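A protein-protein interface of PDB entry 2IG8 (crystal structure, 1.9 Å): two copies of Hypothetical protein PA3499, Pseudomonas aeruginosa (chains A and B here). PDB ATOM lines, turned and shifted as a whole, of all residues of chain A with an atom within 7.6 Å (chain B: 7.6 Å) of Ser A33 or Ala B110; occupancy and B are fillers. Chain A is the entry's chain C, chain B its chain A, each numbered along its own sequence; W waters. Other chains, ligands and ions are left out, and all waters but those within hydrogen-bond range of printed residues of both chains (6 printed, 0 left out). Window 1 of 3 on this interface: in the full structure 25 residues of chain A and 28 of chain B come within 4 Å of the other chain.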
ATOM      1  N   ASP A  14       6.485  20.012   4.261  1.00  0.00           N
ATOM      2  CA  ASP A  14       6.152  19.898   2.857  1.00  0.00           C
ATOM      3  C   ASP A  14       4.712  20.373   2.682  1.00  0.00           C
ATOM      4  O   ASP A  14       3.744  19.714   3.074  1.00  0.00           O
ATOM      5  CB  ASP A  14       6.475  18.505   2.317  1.00  0.00           C
ATOM      6  CG  ASP A  14       7.967  18.356   2.047  1.00  0.00           C
ATOM      7  OD1 ASP A  14       8.457  19.105   1.169  1.00  0.00           O
ATOM      8  OD2 ASP A  14       8.655  17.567   2.740  1.00  0.00           O
ATOM      9  N   SER A  19       5.583  19.739  -5.008  1.00  0.00           N
ATOM     10  CA  SER A  19       5.745  18.468  -5.692  1.00  0.00           C
ATOM     11  C   SER A  19       7.130  17.851  -5.400  1.00  0.00           C
ATOM     12  O   SER A  19       7.783  17.291  -6.294  1.00  0.00           O
ATOM     13  CB  SER A  19       5.503  18.661  -7.188  1.00  0.00           C
ATOM     14  OG  SER A  19       6.295  19.718  -7.702  1.00  0.00           O
ATOM     15  N   TRP A  20       7.571  17.972  -4.145  1.00  0.00           N
ATOM     16  CA  TRP A  20       8.812  17.337  -3.686  1.00  0.00           C
ATOM     17  C   TRP A  20       8.779  17.051  -2.193  1.00  0.00           C
ATOM     18  O   TRP A  20       8.030  17.678  -1.452  1.00  0.00           O
ATOM     19  CB  TRP A  20      10.033  18.206  -4.012  1.00  0.00           C
ATOM     20  CG  TRP A  20      10.022  19.506  -3.314  1.00  0.00           C
ATOM     21  CD1 TRP A  20      10.549  19.783  -2.087  1.00  0.00           C
ATOM     22  CD2 TRP A  20       9.433  20.719  -3.784  1.00  0.00           C
ATOM     23  NE1 TRP A  20      10.336  21.091  -1.773  1.00  0.00           N
ATOM     24  CE2 TRP A  20       9.644  21.692  -2.790  1.00  0.00           C
ATOM     25  CE3 TRP A  20       8.734  21.074  -4.944  1.00  0.00           C
ATOM     26  CZ2 TRP A  20       9.184  23.005  -2.916  1.00  0.00           C
ATOM     27  CZ3 TRP A  20       8.289  22.384  -5.076  1.00  0.00           C
ATOM     28  CH2 TRP A  20       8.514  23.330  -4.068  1.00  0.00           C
ATOM     29  N   SER A  21       9.617  16.114  -1.764  1.00  0.00           N
ATOM     30  CA  SER A  21       9.830  15.836  -0.349  1.00  0.00           C
ATOM     31  C   SER A  21      11.147  16.465   0.085  1.00  0.00           C
ATOM     32  O   SER A  21      12.165  16.307  -0.577  1.00  0.00           O
ATOM     33  CB  SER A  21       9.872  14.330  -0.089  1.00  0.00           C
ATOM     34  OG  SER A  21       8.585  13.746  -0.223  1.00  0.00           O
ATOM     35  N   ASN A  22      11.136  17.153   1.215  1.00  0.00           N
ATOM     36  CA  ASN A  22      12.354  17.786   1.728  1.00  0.00           C
ATOM     37  C   ASN A  22      13.412  16.752   2.109  1.00  0.00           C
ATOM     38  O   ASN A  22      14.615  16.966   1.866  1.00  0.00           O
ATOM     39  CB  ASN A  22      12.039  18.691   2.928  1.00  0.00           C
ATOM     40  CG  ASN A  22      11.459  20.040   2.518  1.00  0.00           C
ATOM     41  OD1 ASN A  22      10.784  20.702   3.312  1.00  0.00           O
ATOM     42  ND2 ASN A  22      11.717  20.454   1.282  1.00  0.00           N
ATOM     43  N   ALA A  23      12.968  15.618   2.654  1.00  0.00           N
ATOM     44  CA  ALA A  23      13.887  14.574   3.112  1.00  0.00           C
ATOM     45  C   ALA A  23      13.230  13.202   3.118  1.00  0.00           C
ATOM     46  O   ALA A  23      12.129  13.036   3.629  1.00  0.00           O
ATOM     47  CB  ALA A  23      14.409  14.909   4.527  1.00  0.00           C
ATOM     48  N   LEU A  24      13.929  12.214   2.569  1.00  0.00           N
ATOM     49  CA  LEU A  24      13.453  10.836   2.546  1.00  0.00           C
ATOM     50  C   LEU A  24      14.600   9.951   3.006  1.00  0.00           C
ATOM     51  O   LEU A  24      15.713  10.046   2.465  1.00  0.00           O
ATOM     52  CB  LEU A  24      13.065  10.455   1.126  1.00  0.00           C
ATOM     53  CG  LEU A  24      11.923  11.234   0.466  1.00  0.00           C
ATOM     54  CD1 LEU A  24      11.977  10.988  -1.068  1.00  0.00           C
ATOM     55  CD2 LEU A  24      10.567  10.845   1.073  1.00  0.00           C
ATOM     56  N   LEU A  30      20.162   9.381   3.539  1.00  0.00           N
ATOM     57  CA  LEU A  30      19.210  10.476   3.756  1.00  0.00           C
ATOM     58  C   LEU A  30      19.210  11.345   2.532  1.00  0.00           C
ATOM     59  O   LEU A  30      20.138  12.114   2.308  1.00  0.00           O
ATOM     60  CB  LEU A  30      19.510  11.321   5.010  1.00  0.00           C
ATOM     61  CG  LEU A  30      18.429  12.372   5.356  1.00  0.00           C
ATOM     62  CD1 LEU A  30      17.110  11.752   5.800  1.00  0.00           C
ATOM     63  CD2 LEU A  30      18.916  13.342   6.427  1.00  0.00           C
ATOM     64  N   VAL A  31      18.163  11.206   1.738  1.00  0.00           N
ATOM     65  CA  VAL A  31      18.034  11.908   0.457  1.00  0.00           C
ATOM     66  C   VAL A  31      17.380  13.237   0.792  1.00  0.00           C
ATOM     67  O   VAL A  31      16.370  13.258   1.480  1.00  0.00           O
ATOM     68  CB  VAL A  31      17.164  11.123  -0.529  1.00  0.00           C
ATOM     69  CG1 VAL A  31      17.036  11.871  -1.855  1.00  0.00           C
ATOM     70  CG2 VAL A  31      17.749   9.724  -0.766  1.00  0.00           C
ATOM     71  N   MET A  32      17.948  14.341   0.322  1.00  0.00           N
ATOM     72  CA  MET A  32      17.454  15.659   0.704  1.00  0.00           C
ATOM     73  C   MET A  32      17.168  16.518  -0.518  1.00  0.00           C
ATOM     74  O   MET A  32      17.882  16.425  -1.502  1.00  0.00           O
ATOM     75  CB  MET A  32      18.484  16.360   1.613  1.00  0.00           C
ATOM     76  CG  MET A  32      18.519  15.825   3.062  1.00  0.00           C
ATOM     77  SD  MET A  32      19.798  16.553   4.159  1.00  0.00           S
ATOM     78  CE  MET A  32      21.154  15.432   3.855  1.00  0.00           C
ATOM     79  N   SER A  33      16.142  17.369  -0.445  1.00  0.00           N
ATOM     80  CA  SER A  33      15.935  18.379  -1.480  1.00  0.00           C
ATOM     81  C   SER A  33      16.979  19.481  -1.269  1.00  0.00           C
ATOM     82  O   SER A  33      17.528  19.604  -0.179  1.00  0.00           O
ATOM     83  CB  SER A  33      14.532  18.980  -1.446  1.00  0.00           C
ATOM     84  OG  SER A  33      13.545  18.066  -1.913  1.00  0.00           O
ATOM     85  N   GLY A  34      17.235  20.255  -2.317  1.00  0.00           N
ATOM     86  CA  GLY A  34      18.086  21.430  -2.244  1.00  0.00           C
ATOM     87  C   GLY A  34      17.551  22.414  -1.242  1.00  0.00           C
ATOM     88  O   GLY A  34      16.330  22.634  -1.157  1.00  0.00           O
ATOM     89  N   MET A  35      18.446  22.978  -0.447  1.00  0.00           N
ATOM     90  CA  MET A  35      18.038  23.855   0.620  1.00  0.00           C
ATOM     91  C   MET A  35      18.521  25.269   0.349  1.00  0.00           C
ATOM     92  O   MET A  35      19.601  25.489  -0.231  1.00  0.00           O
ATOM     93  CB  MET A  35      18.529  23.344   1.981  1.00  0.00           C
ATOM     94  CG  MET A  35      17.836  22.048   2.468  1.00  0.00           C
ATOM     95  SD  MET A  35      16.203  22.177   3.247  1.00  0.00           S
ATOM     96  CE  MET A  35      15.531  23.762   2.716  1.00  0.00           C
ATOM     97  N   THR A  36      17.681  26.208   0.771  1.00  0.00           N
ATOM     98  CA  THR A  36      17.928  27.624   0.603  1.00  0.00           C
ATOM     99  C   THR A  36      17.622  28.345   1.909  1.00  0.00           C
ATOM    100  O   THR A  36      16.996  27.791   2.821  1.00  0.00           O
ATOM    101  CB  THR A  36      17.067  28.241  -0.518  1.00  0.00           C
ATOM    102  OG1 THR A  36      15.739  28.473  -0.045  1.00  0.00           O
ATOM    103  CG2 THR A  36      17.029  27.320  -1.767  1.00  0.00           C
ATOM    104  N   VAL A  64      20.049  21.744   6.568  1.00  0.00           N
ATOM    105  CA  VAL A  64      20.585  20.410   6.337  1.00  0.00           C
ATOM    106  C   VAL A  64      20.788  19.696   7.680  1.00  0.00           C
ATOM    107  O   VAL A  64      20.409  18.528   7.824  1.00  0.00           O
ATOM    108  CB  VAL A  64      21.886  20.434   5.474  1.00  0.00           C
ATOM    109  CG1 VAL A  64      22.474  19.050   5.371  1.00  0.00           C
ATOM    110  CG2 VAL A  64      21.592  20.984   4.087  1.00  0.00           C
ATOM    111  N   LEU A  67      17.345  18.541   9.091  1.00  0.00           N
ATOM    112  CA  LEU A  67      16.893  17.345   8.384  1.00  0.00           C
ATOM    113  C   LEU A  67      17.646  16.121   8.906  1.00  0.00           C
ATOM    114  O   LEU A  67      17.005  15.133   9.341  1.00  0.00           O
ATOM    115  CB  LEU A  67      17.051  17.520   6.871  1.00  0.00           C
ATOM    116  CG  LEU A  67      16.098  18.548   6.235  1.00  0.00           C
ATOM    117  CD1 LEU A  67      16.444  18.801   4.789  1.00  0.00           C
ATOM    118  CD2 LEU A  67      14.633  18.114   6.353  1.00  0.00           C
ATOM    119  N   GLU A 127      22.151  27.833  -3.058  1.00  0.00           N
ATOM    120  CA  GLU A 127      21.355  26.640  -2.761  1.00  0.00           C
ATOM    121  C   GLU A 127      22.315  25.466  -2.649  1.00  0.00           C
ATOM    122  O   GLU A 127      23.276  25.380  -3.433  1.00  0.00           O
ATOM    123  CB  GLU A 127      20.295  26.405  -3.837  1.00  0.00           C
ATOM    124  CG  GLU A 127      19.400  25.181  -3.585  1.00  0.00           C
ATOM    125  CD  GLU A 127      18.057  25.210  -4.315  1.00  0.00           C
ATOM    126  OE1 GLU A 127      17.708  26.196  -5.003  1.00  0.00           O
ATOM    127  OE2 GLU A 127      17.328  24.209  -4.200  1.00  0.00           O
ATOM    128  N   ILE A 128      22.110  24.602  -1.657  1.00  0.00           N
ATOM    129  CA  ILE A 128      22.967  23.430  -1.470  1.00  0.00           C
ATOM    130  C   ILE A 128      22.166  22.130  -1.540  1.00  0.00           C
ATOM    131  O   ILE A 128      21.182  21.956  -0.817  1.00  0.00           O
ATOM    132  CB  ILE A 128      23.799  23.470  -0.168  1.00  0.00           C
ATOM    133  CG1 ILE A 128      24.719  24.705  -0.149  1.00  0.00           C
ATOM    134  CG2 ILE A 128      24.628  22.175  -0.046  1.00  0.00           C
ATOM    135  CD1 ILE A 128      25.581  24.863   1.139  1.00  0.00           C
ATOM    136  N   ASP A 129      22.579  21.251  -2.450  1.00  0.00           N
ATOM    137  CA  ASP A 129      22.077  19.884  -2.515  1.00  0.00           C
ATOM    138  C   ASP A 129      23.070  19.020  -1.717  1.00  0.00           C
ATOM    139  O   ASP A 129      24.242  18.872  -2.109  1.00  0.00           O
ATOM    140  CB  ASP A 129      21.975  19.461  -3.989  1.00  0.00           C
ATOM    141  CG  ASP A 129      21.260  18.136  -4.215  1.00  0.00           C
ATOM    142  OD1 ASP A 129      20.674  17.522  -3.294  1.00  0.00           O
ATOM    143  OD2 ASP A 129      21.309  17.672  -5.383  1.00  0.00           O
ATOM    144  N   ALA A 130      22.609  18.486  -0.582  1.00  0.00           N
ATOM    145  CA  ALA A 130      23.451  17.692   0.321  1.00  0.00           C
ATOM    146  C   ALA A 130      23.170  16.198   0.212  1.00  0.00           C
ATOM    147  O   ALA A 130      22.034  15.795  -0.017  1.00  0.00           O
ATOM    148  CB  ALA A 130      23.256  18.151   1.761  1.00  0.00           C
ATOM    149  N   LEU B  78      11.678   6.262  -8.089  1.00  0.00           N
ATOM    150  CA  LEU B  78      12.353   7.563  -8.094  1.00  0.00           C
ATOM    151  C   LEU B  78      12.468   8.137  -6.679  1.00  0.00           C
ATOM    152  O   LEU B  78      11.493   8.186  -5.955  1.00  0.00           O
ATOM    153  CB  LEU B  78      11.608   8.560  -8.997  1.00  0.00           C
ATOM    154  CG  LEU B  78      11.628   8.294 -10.499  1.00  0.00           C
ATOM    155  CD1 LEU B  78      10.472   8.981 -11.247  1.00  0.00           C
ATOM    156  CD2 LEU B  78      12.987   8.718 -11.087  1.00  0.00           C
ATOM    157  N   TYR B  79      13.669   8.593  -6.300  1.00  0.00           N
ATOM    158  CA  TYR B  79      13.863   9.242  -4.997  1.00  0.00           C
ATOM    159  C   TYR B  79      14.396  10.674  -5.107  1.00  0.00           C
ATOM    160  O   TYR B  79      14.271  11.436  -4.166  1.00  0.00           O
ATOM    161  CB  TYR B  79      14.738   8.386  -4.069  1.00  0.00           C
ATOM    162  CG  TYR B  79      16.137   8.136  -4.555  1.00  0.00           C
ATOM    163  CD1 TYR B  79      17.140   9.056  -4.308  1.00  0.00           C
ATOM    164  CD2 TYR B  79      16.464   6.977  -5.269  1.00  0.00           C
ATOM    165  CE1 TYR B  79      18.427   8.858  -4.771  1.00  0.00           C
ATOM    166  CE2 TYR B  79      17.774   6.760  -5.716  1.00  0.00           C
ATOM    167  CZ  TYR B  79      18.744   7.705  -5.446  1.00  0.00           C
ATOM    168  OH  TYR B  79      20.039   7.558  -5.869  1.00  0.00           O
ATOM    169  N   LYS B  80      14.979  11.047  -6.242  1.00  0.00           N
ATOM    170  CA  LYS B  80      15.444  12.424  -6.411  1.00  0.00           C
ATOM    171  C   LYS B  80      15.363  12.864  -7.862  1.00  0.00           C
ATOM    172  O   LYS B  80      15.638  12.067  -8.783  1.00  0.00           O
ATOM    173  CB  LYS B  80      16.857  12.594  -5.850  1.00  0.00           C
ATOM    174  CG  LYS B  80      17.284  14.068  -5.725  1.00  0.00           C
ATOM    175  CD  LYS B  80      18.757  14.247  -5.378  1.00  0.00           C
ATOM    176  CE  LYS B  80      19.035  14.191  -3.905  1.00  0.00           C
ATOM    177  NZ  LYS B  80      20.147  15.102  -3.513  1.00  0.00           N
ATOM    178  N   LEU B  81      14.924  14.111  -8.050  1.00  0.00           N
ATOM    179  CA  LEU B  81      14.897  14.769  -9.349  1.00  0.00           C
ATOM    180  C   LEU B  81      15.697  16.078  -9.296  1.00  0.00           C
ATOM    181  O   LEU B  81      15.336  17.000  -8.590  1.00  0.00           O
ATOM    182  CB  LEU B  81      13.466  15.092  -9.787  1.00  0.00           C
ATOM    183  CG  LEU B  81      12.494  13.921  -9.916  1.00  0.00           C
ATOM    184  CD1 LEU B  81      11.148  14.462 -10.334  1.00  0.00           C
ATOM    185  CD2 LEU B  81      13.012  12.865 -10.925  1.00  0.00           C
ATOM    186  N   ASN B  82      16.779  16.140 -10.058  1.00  0.00           N
ATOM    187  CA  ASN B  82      17.514  17.396 -10.287  1.00  0.00           C
ATOM    188  C   ASN B  82      16.998  18.034 -11.569  1.00  0.00           C
ATOM    189  O   ASN B  82      17.140  17.447 -12.668  1.00  0.00           O
ATOM    190  CB  ASN B  82      19.013  17.121 -10.384  1.00  0.00           C
ATOM    191  CG  ASN B  82      19.673  16.999  -9.027  1.00  0.00           C
ATOM    192  OD1 ASN B  82      20.061  18.002  -8.429  1.00  0.00           O
ATOM    193  ND2 ASN B  82      19.833  15.778  -8.546  1.00  0.00           N
ATOM    194  N   VAL B  83      16.378  19.202 -11.431  1.00  0.00           N
ATOM    195  CA  VAL B  83      15.743  19.915 -12.538  1.00  0.00           C
ATOM    196  C   VAL B  83      16.544  21.156 -12.888  1.00  0.00           C
ATOM    197  O   VAL B  83      16.835  21.986 -12.022  1.00  0.00           O
ATOM    198  CB  VAL B  83      14.286  20.320 -12.194  1.00  0.00           C
ATOM    199  CG1 VAL B  83      13.570  20.916 -13.412  1.00  0.00           C
ATOM    200  CG2 VAL B  83      13.523  19.136 -11.628  1.00  0.00           C
ATOM    201  N   ARG B  98       4.782  17.664 -12.383  1.00  0.00           N
ATOM    202  CA  ARG B  98       5.100  16.635 -11.390  1.00  0.00           C
ATOM    203  C   ARG B  98       3.841  16.147 -10.677  1.00  0.00           C
ATOM    204  O   ARG B  98       3.704  14.960 -10.405  1.00  0.00           O
ATOM    205  CB  ARG B  98       6.084  17.141 -10.350  1.00  0.00           C
ATOM    206  CG  ARG B  98       7.511  17.162 -10.827  1.00  0.00           C
ATOM    207  CD  ARG B  98       8.478  17.368  -9.695  1.00  0.00           C
ATOM    208  NE  ARG B  98       8.605  18.787  -9.365  1.00  0.00           N
ATOM    209  CZ  ARG B  98       9.718  19.364  -8.922  1.00  0.00           C
ATOM    210  NH1 ARG B  98      10.820  18.660  -8.711  1.00  0.00           N
ATOM    211  NH2 ARG B  98       9.717  20.661  -8.674  1.00  0.00           N
ATOM    212  N   THR B 107       3.830  10.290  -1.939  1.00  0.00           N
ATOM    213  CA  THR B 107       5.036  10.949  -1.533  1.00  0.00           C
ATOM    214  C   THR B 107       5.827  11.267  -2.779  1.00  0.00           C
ATOM    215  O   THR B 107       5.909  10.425  -3.660  1.00  0.00           O
ATOM    216  CB  THR B 107       5.824   9.989  -0.658  1.00  0.00           C
ATOM    217  OG1 THR B 107       5.029   9.659   0.493  1.00  0.00           O
ATOM    218  CG2 THR B 107       7.157  10.596  -0.243  1.00  0.00           C
ATOM    219  N   PHE B 108       6.367  12.482  -2.859  1.00  0.00           N
ATOM    220  CA  PHE B 108       7.156  12.915  -4.019  1.00  0.00           C
ATOM    221  C   PHE B 108       8.642  12.663  -3.778  1.00  0.00           C
ATOM    222  O   PHE B 108       9.108  12.692  -2.634  1.00  0.00           O
ATOM    223  CB  PHE B 108       6.982  14.421  -4.288  1.00  0.00           C
ATOM    224  CG  PHE B 108       5.635  14.795  -4.855  1.00  0.00           C
ATOM    225  CD1 PHE B 108       5.395  14.711  -6.224  1.00  0.00           C
ATOM    226  CD2 PHE B 108       4.621  15.261  -4.022  1.00  0.00           C
ATOM    227  CE1 PHE B 108       4.145  15.058  -6.757  1.00  0.00           C
ATOM    228  CE2 PHE B 108       3.365  15.604  -4.544  1.00  0.00           C
ATOM    229  CZ  PHE B 108       3.135  15.496  -5.923  1.00  0.00           C
ATOM    230  N   PRO B 109       9.400  12.440  -4.851  1.00  0.00           N
ATOM    231  CA  PRO B 109      10.851  12.424  -4.722  1.00  0.00           C
ATOM    232  C   PRO B 109      11.398  13.761  -4.188  1.00  0.00           C
ATOM    233  O   PRO B 109      10.722  14.791  -4.261  1.00  0.00           O
ATOM    234  CB  PRO B 109      11.338  12.199  -6.159  1.00  0.00           C
ATOM    235  CG  PRO B 109      10.204  11.724  -6.907  1.00  0.00           C
ATOM    236  CD  PRO B 109       8.962  12.164  -6.231  1.00  0.00           C
ATOM    237  N   ALA B 110      12.606  13.719  -3.644  1.00  0.00           N
ATOM    238  CA  ALA B 110      13.329  14.945  -3.332  1.00  0.00           C
ATOM    239  C   ALA B 110      13.642  15.672  -4.635  1.00  0.00           C
ATOM    240  O   ALA B 110      13.608  15.091  -5.729  1.00  0.00           O
ATOM    241  CB  ALA B 110      14.616  14.651  -2.558  1.00  0.00           C
ATOM    242  N   SER B 111      13.940  16.954  -4.518  1.00  0.00           N
ATOM    243  CA  SER B 111      14.202  17.762  -5.691  1.00  0.00           C
ATOM    244  C   SER B 111      15.133  18.934  -5.453  1.00  0.00           C
ATOM    245  O   SER B 111      15.065  19.587  -4.418  1.00  0.00           O
ATOM    246  CB  SER B 111      12.899  18.358  -6.218  1.00  0.00           C
ATOM    247  OG  SER B 111      13.184  18.996  -7.459  1.00  0.00           O
ATOM    248  N   THR B 112      15.940  19.232  -6.463  1.00  0.00           N
ATOM    249  CA  THR B 112      16.619  20.516  -6.585  1.00  0.00           C
ATOM    250  C   THR B 112      16.331  21.087  -7.977  1.00  0.00           C
ATOM    251  O   THR B 112      16.469  20.372  -8.991  1.00  0.00           O
ATOM    252  CB  THR B 112      18.139  20.367  -6.374  1.00  0.00           C
ATOM    253  OG1 THR B 112      18.381  19.889  -5.049  1.00  0.00           O
ATOM    254  CG2 THR B 112      18.853  21.695  -6.551  1.00  0.00           C
ATOM    255  N   LEU B 113      15.931  22.356  -8.023  1.00  0.00           N
ATOM    256  CA  LEU B 113      15.624  23.059  -9.263  1.00  0.00           C
ATOM    257  C   LEU B 113      16.376  24.377  -9.314  1.00  0.00           C
ATOM    258  O   LEU B 113      16.211  25.237  -8.430  1.00  0.00           O
ATOM    259  CB  LEU B 113      14.120  23.308  -9.412  1.00  0.00           C
ATOM    260  CG  LEU B 113      13.559  23.879 -10.734  1.00  0.00           C
ATOM    261  CD1 LEU B 113      12.090  23.408 -10.888  1.00  0.00           C
ATOM    262  CD2 LEU B 113      13.613  25.407 -10.792  1.00  0.00           C
ATOM    263  N   ASP B 129      17.716  15.341 -14.386  1.00  0.00           N
ATOM    264  CA  ASP B 129      18.614  14.271 -13.958  1.00  0.00           C
ATOM    265  C   ASP B 129      17.903  13.525 -12.825  1.00  0.00           C
ATOM    266  O   ASP B 129      17.724  14.055 -11.706  1.00  0.00           O
ATOM    267  CB  ASP B 129      19.945  14.855 -13.509  1.00  0.00           C
ATOM    268  CG  ASP B 129      21.000  13.787 -13.183  1.00  0.00           C
ATOM    269  OD1 ASP B 129      20.837  12.599 -13.575  1.00  0.00           O
ATOM    270  OD2 ASP B 129      21.998  14.162 -12.503  1.00  0.00           O
ATOM    271  N   TRP B 131      17.033  10.180 -10.303  1.00  0.00           N
ATOM    272  CA  TRP B 131      17.701   9.184  -9.490  1.00  0.00           C
ATOM    273  C   TRP B 131      16.649   8.209  -8.975  1.00  0.00           C
ATOM    274  O   TRP B 131      15.639   8.630  -8.400  1.00  0.00           O
ATOM    275  CB  TRP B 131      18.415   9.821  -8.302  1.00  0.00           C
ATOM    276  CG  TRP B 131      19.455  10.871  -8.640  1.00  0.00           C
ATOM    277  CD1 TRP B 131      19.231  12.186  -8.907  1.00  0.00           C
ATOM    278  CD2 TRP B 131      20.873  10.680  -8.697  1.00  0.00           C
ATOM    279  NE1 TRP B 131      20.432  12.832  -9.156  1.00  0.00           N
ATOM    280  CE2 TRP B 131      21.451  11.923  -9.042  1.00  0.00           C
ATOM    281  CE3 TRP B 131      21.713   9.568  -8.524  1.00  0.00           C
ATOM    282  CZ2 TRP B 131      22.843  12.095  -9.195  1.00  0.00           C
ATOM    283  CZ3 TRP B 131      23.114   9.739  -8.701  1.00  0.00           C
ATOM    284  CH2 TRP B 131      23.650  10.990  -9.028  1.00  0.00           C
ATOM    285  N   LEU B 138       8.076   4.628  -3.334  1.00  0.00           N
ATOM    286  CA  LEU B 138       7.637   5.789  -2.561  1.00  0.00           C
ATOM    287  C   LEU B 138       6.145   5.740  -2.292  1.00  0.00           C
ATOM    288  O   LEU B 138       5.672   6.435  -1.404  1.00  0.00           O
ATOM    289  CB  LEU B 138       8.003   7.124  -3.234  1.00  0.00           C
ATOM    290  CG  LEU B 138       9.355   7.718  -2.831  1.00  0.00           C
ATOM    291  CD1 LEU B 138      10.465   6.753  -3.146  1.00  0.00           C
ATOM    292  CD2 LEU B 138       9.575   9.076  -3.491  1.00  0.00           C
HETATM  293  O   HOH W   1      18.214  17.091  -4.331  1.00  0.00           O
HETATM  294  O   HOH W   2      16.724  27.341  -6.954  1.00  0.00           O
HETATM  295  O   HOH W   3      15.349  24.032  -5.724  1.00  0.00           O
HETATM  296  O   HOH W   4       5.972  14.278  -0.738  1.00  0.00           O
HETATM  297  O   HOH W   5      20.584  13.677  -1.019  1.00  0.00           O
HETATM  298  O   HOH W   6      10.044  15.970  -7.018  1.00  0.00           O
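Ser A19 touches Phe B108 (C to CG, 3.4 Å).
Trp A20 touches Pro B109 (CA to O, 3.2 Å).
CB of Trp A20 touches CB of Ser B111, at 3.6 Å.
Ala B110 touches Ser A21 (CA to O, 3.3 Å).
CD1 of Leu A24 touches N of Ala B110, 3.8 Å away.
CD1 of Leu A24 touches CD2 of Leu B138, at 3.9 Å.
Val A31 touches Tyr B79 (CG1 to O, 3.6 Å).
Ala B110 touches Ser A33 (CA to OG, 3.4 Å).
Glu A127 touches Leu B113 (OE1 to O, 3.9 Å).
Asp A129 touches Thr B112 (CG to OG1, 3.5 Å).
The backbone NH (N) of Gly A34 sits at hydrogen-bond distance from the side-chain hydroxyl (OG1) of Thr B112 (3.0 Å).
The backbone NH (N) of Gly A34 sits at hydrogen-bond distance from the backbone carbonyl oxygen (O) of Ser B111.
The side-chain hydroxyl of Ser A33 lies within hydrogen-bond range of the backbone NH of Ser B111 (2.9 Å).
The side-chain amino group (NZ) of Lys B80 is in hydrogen-bond range of the backbone carbonyl oxygen (O) of Met A32 (3.3 Å).
The side-chain amide oxygen (OD1) of Asn B82 lies close to the side-chain carboxylate (OD2) of Asp A129 (3.3 Å).
OD1 of Asp A129 lies within salt-bridge range of NZ of Lys B80 (2.5 Å).
The guanidinium group (NE) of Arg B98 lies within hydrogen-bond range of the side-chain hydroxyl (OG) of Ser A19 (3.0 Å).
The backbone carbonyl oxygen (O) of Phe B108 sits at hydrogen-bond distance from the side-chain hydroxyl (OG) of Ser A21, at 2.7 Å.
N of Ser A21 sits at hydrogen-bond distance from O of Pro B109 (3.0 Å).
Printed residues of chain A that touch a printed residue of chain B: Ser A19, Trp A20, Ser A21, Leu A24, Val A31, Met A32, Ser A33, Gly A34, Glu A127 and Asp A129.
Of the 17 printed residues of chain B, 12 touch a printed residue of chain A.
Printed residues of chain B that touch a printed residue of chain A: Tyr B79, Lys B80, Asn B82, Arg B98, Thr B107, Phe B108, Pro B109, Ala B110, Ser B111, Thr B112, Leu B113 and Leu B138.
Along chain B the printed residues that touch a printed residue of chain A span positions 79 to 138.
Among the printed residues, Asp or Glu carboxylates within 4 Å of a Lys or Arg side-chain nitrogen of the other chain: Asp A129 with Lys B80.
Water W2 lies within hydrogen-bond range of OE1 of Glu A127 (2.5 Å) and O of Leu B113 (2.6 Å).
Water W4 bridges the side-chain hydroxyl of Ser A21 (2.7 Å) and the backbone NH of Phe B108 (2.8 Å).
Water W6 lies within hydrogen-bond range of the backbone carbonyl oxygen of Ser A19 (2.7 Å), the backbone carbonyl oxygen of Pro B109 (3.1 Å) and the guanidinium group of Arg B98 (3.3 Å).
Position printed for both chains: 129.
Of the 29 pairs that touch across the chains among the printed residues, none has its exchanged pair printed and touching as well.
Of chain B, only Ala B110 and Ser B111 come within 4 Å of Ser A33.
Ala B110 touches just these residues of chain A: Ser A21 (3.3 Å), Leu A24 (3.8 Å), Val A31 (3.8 Å), Met A32 (3.8 Å) and Ser A33 (3.4 Å).
Of chain B, only Ser B111 and Thr B112 come within 4 Å of Gly A34.
Printed residues of chain A within 4 Å of Pro B109: Trp A20 (3.2 Å) and Ser A21 (3.0 Å).
Of the printed residues of chain B, Asp A129 touches Lys B80, Asn B82 and Thr B112.
Of the printed residues of chain B, Val A31 touches Tyr B79, Lys B80 and Ala B110.
Printed residues of chain A within 4 Å of Phe B108: Ser A19, Trp A20, Ser A21 and Leu A24.
Asn A22 touches none of the printed residues of chain B.
The nearest residue of chain B that does not touch Ser A33 is Thr B112 (4.1 Å).
The nearest residue of chain A that does not touch Ala B110 is Trp A20 (4.5 Å).
OG of Ser B111 is in hydrogen-bond range of O of Leu B81, at 3.1 Å.
The backbone NH (N) of Val B83 sits at hydrogen-bond distance from the backbone carbonyl oxygen (O) of Thr B112 (2.7 Å).
The backbone carbonyl oxygen (O) of Trp B131 lies within hydrogen-bond range of the backbone NH (N) of Tyr B79 (2.9 Å).
O of Ser A21 is in hydrogen-bond range of OG of Ser A33.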
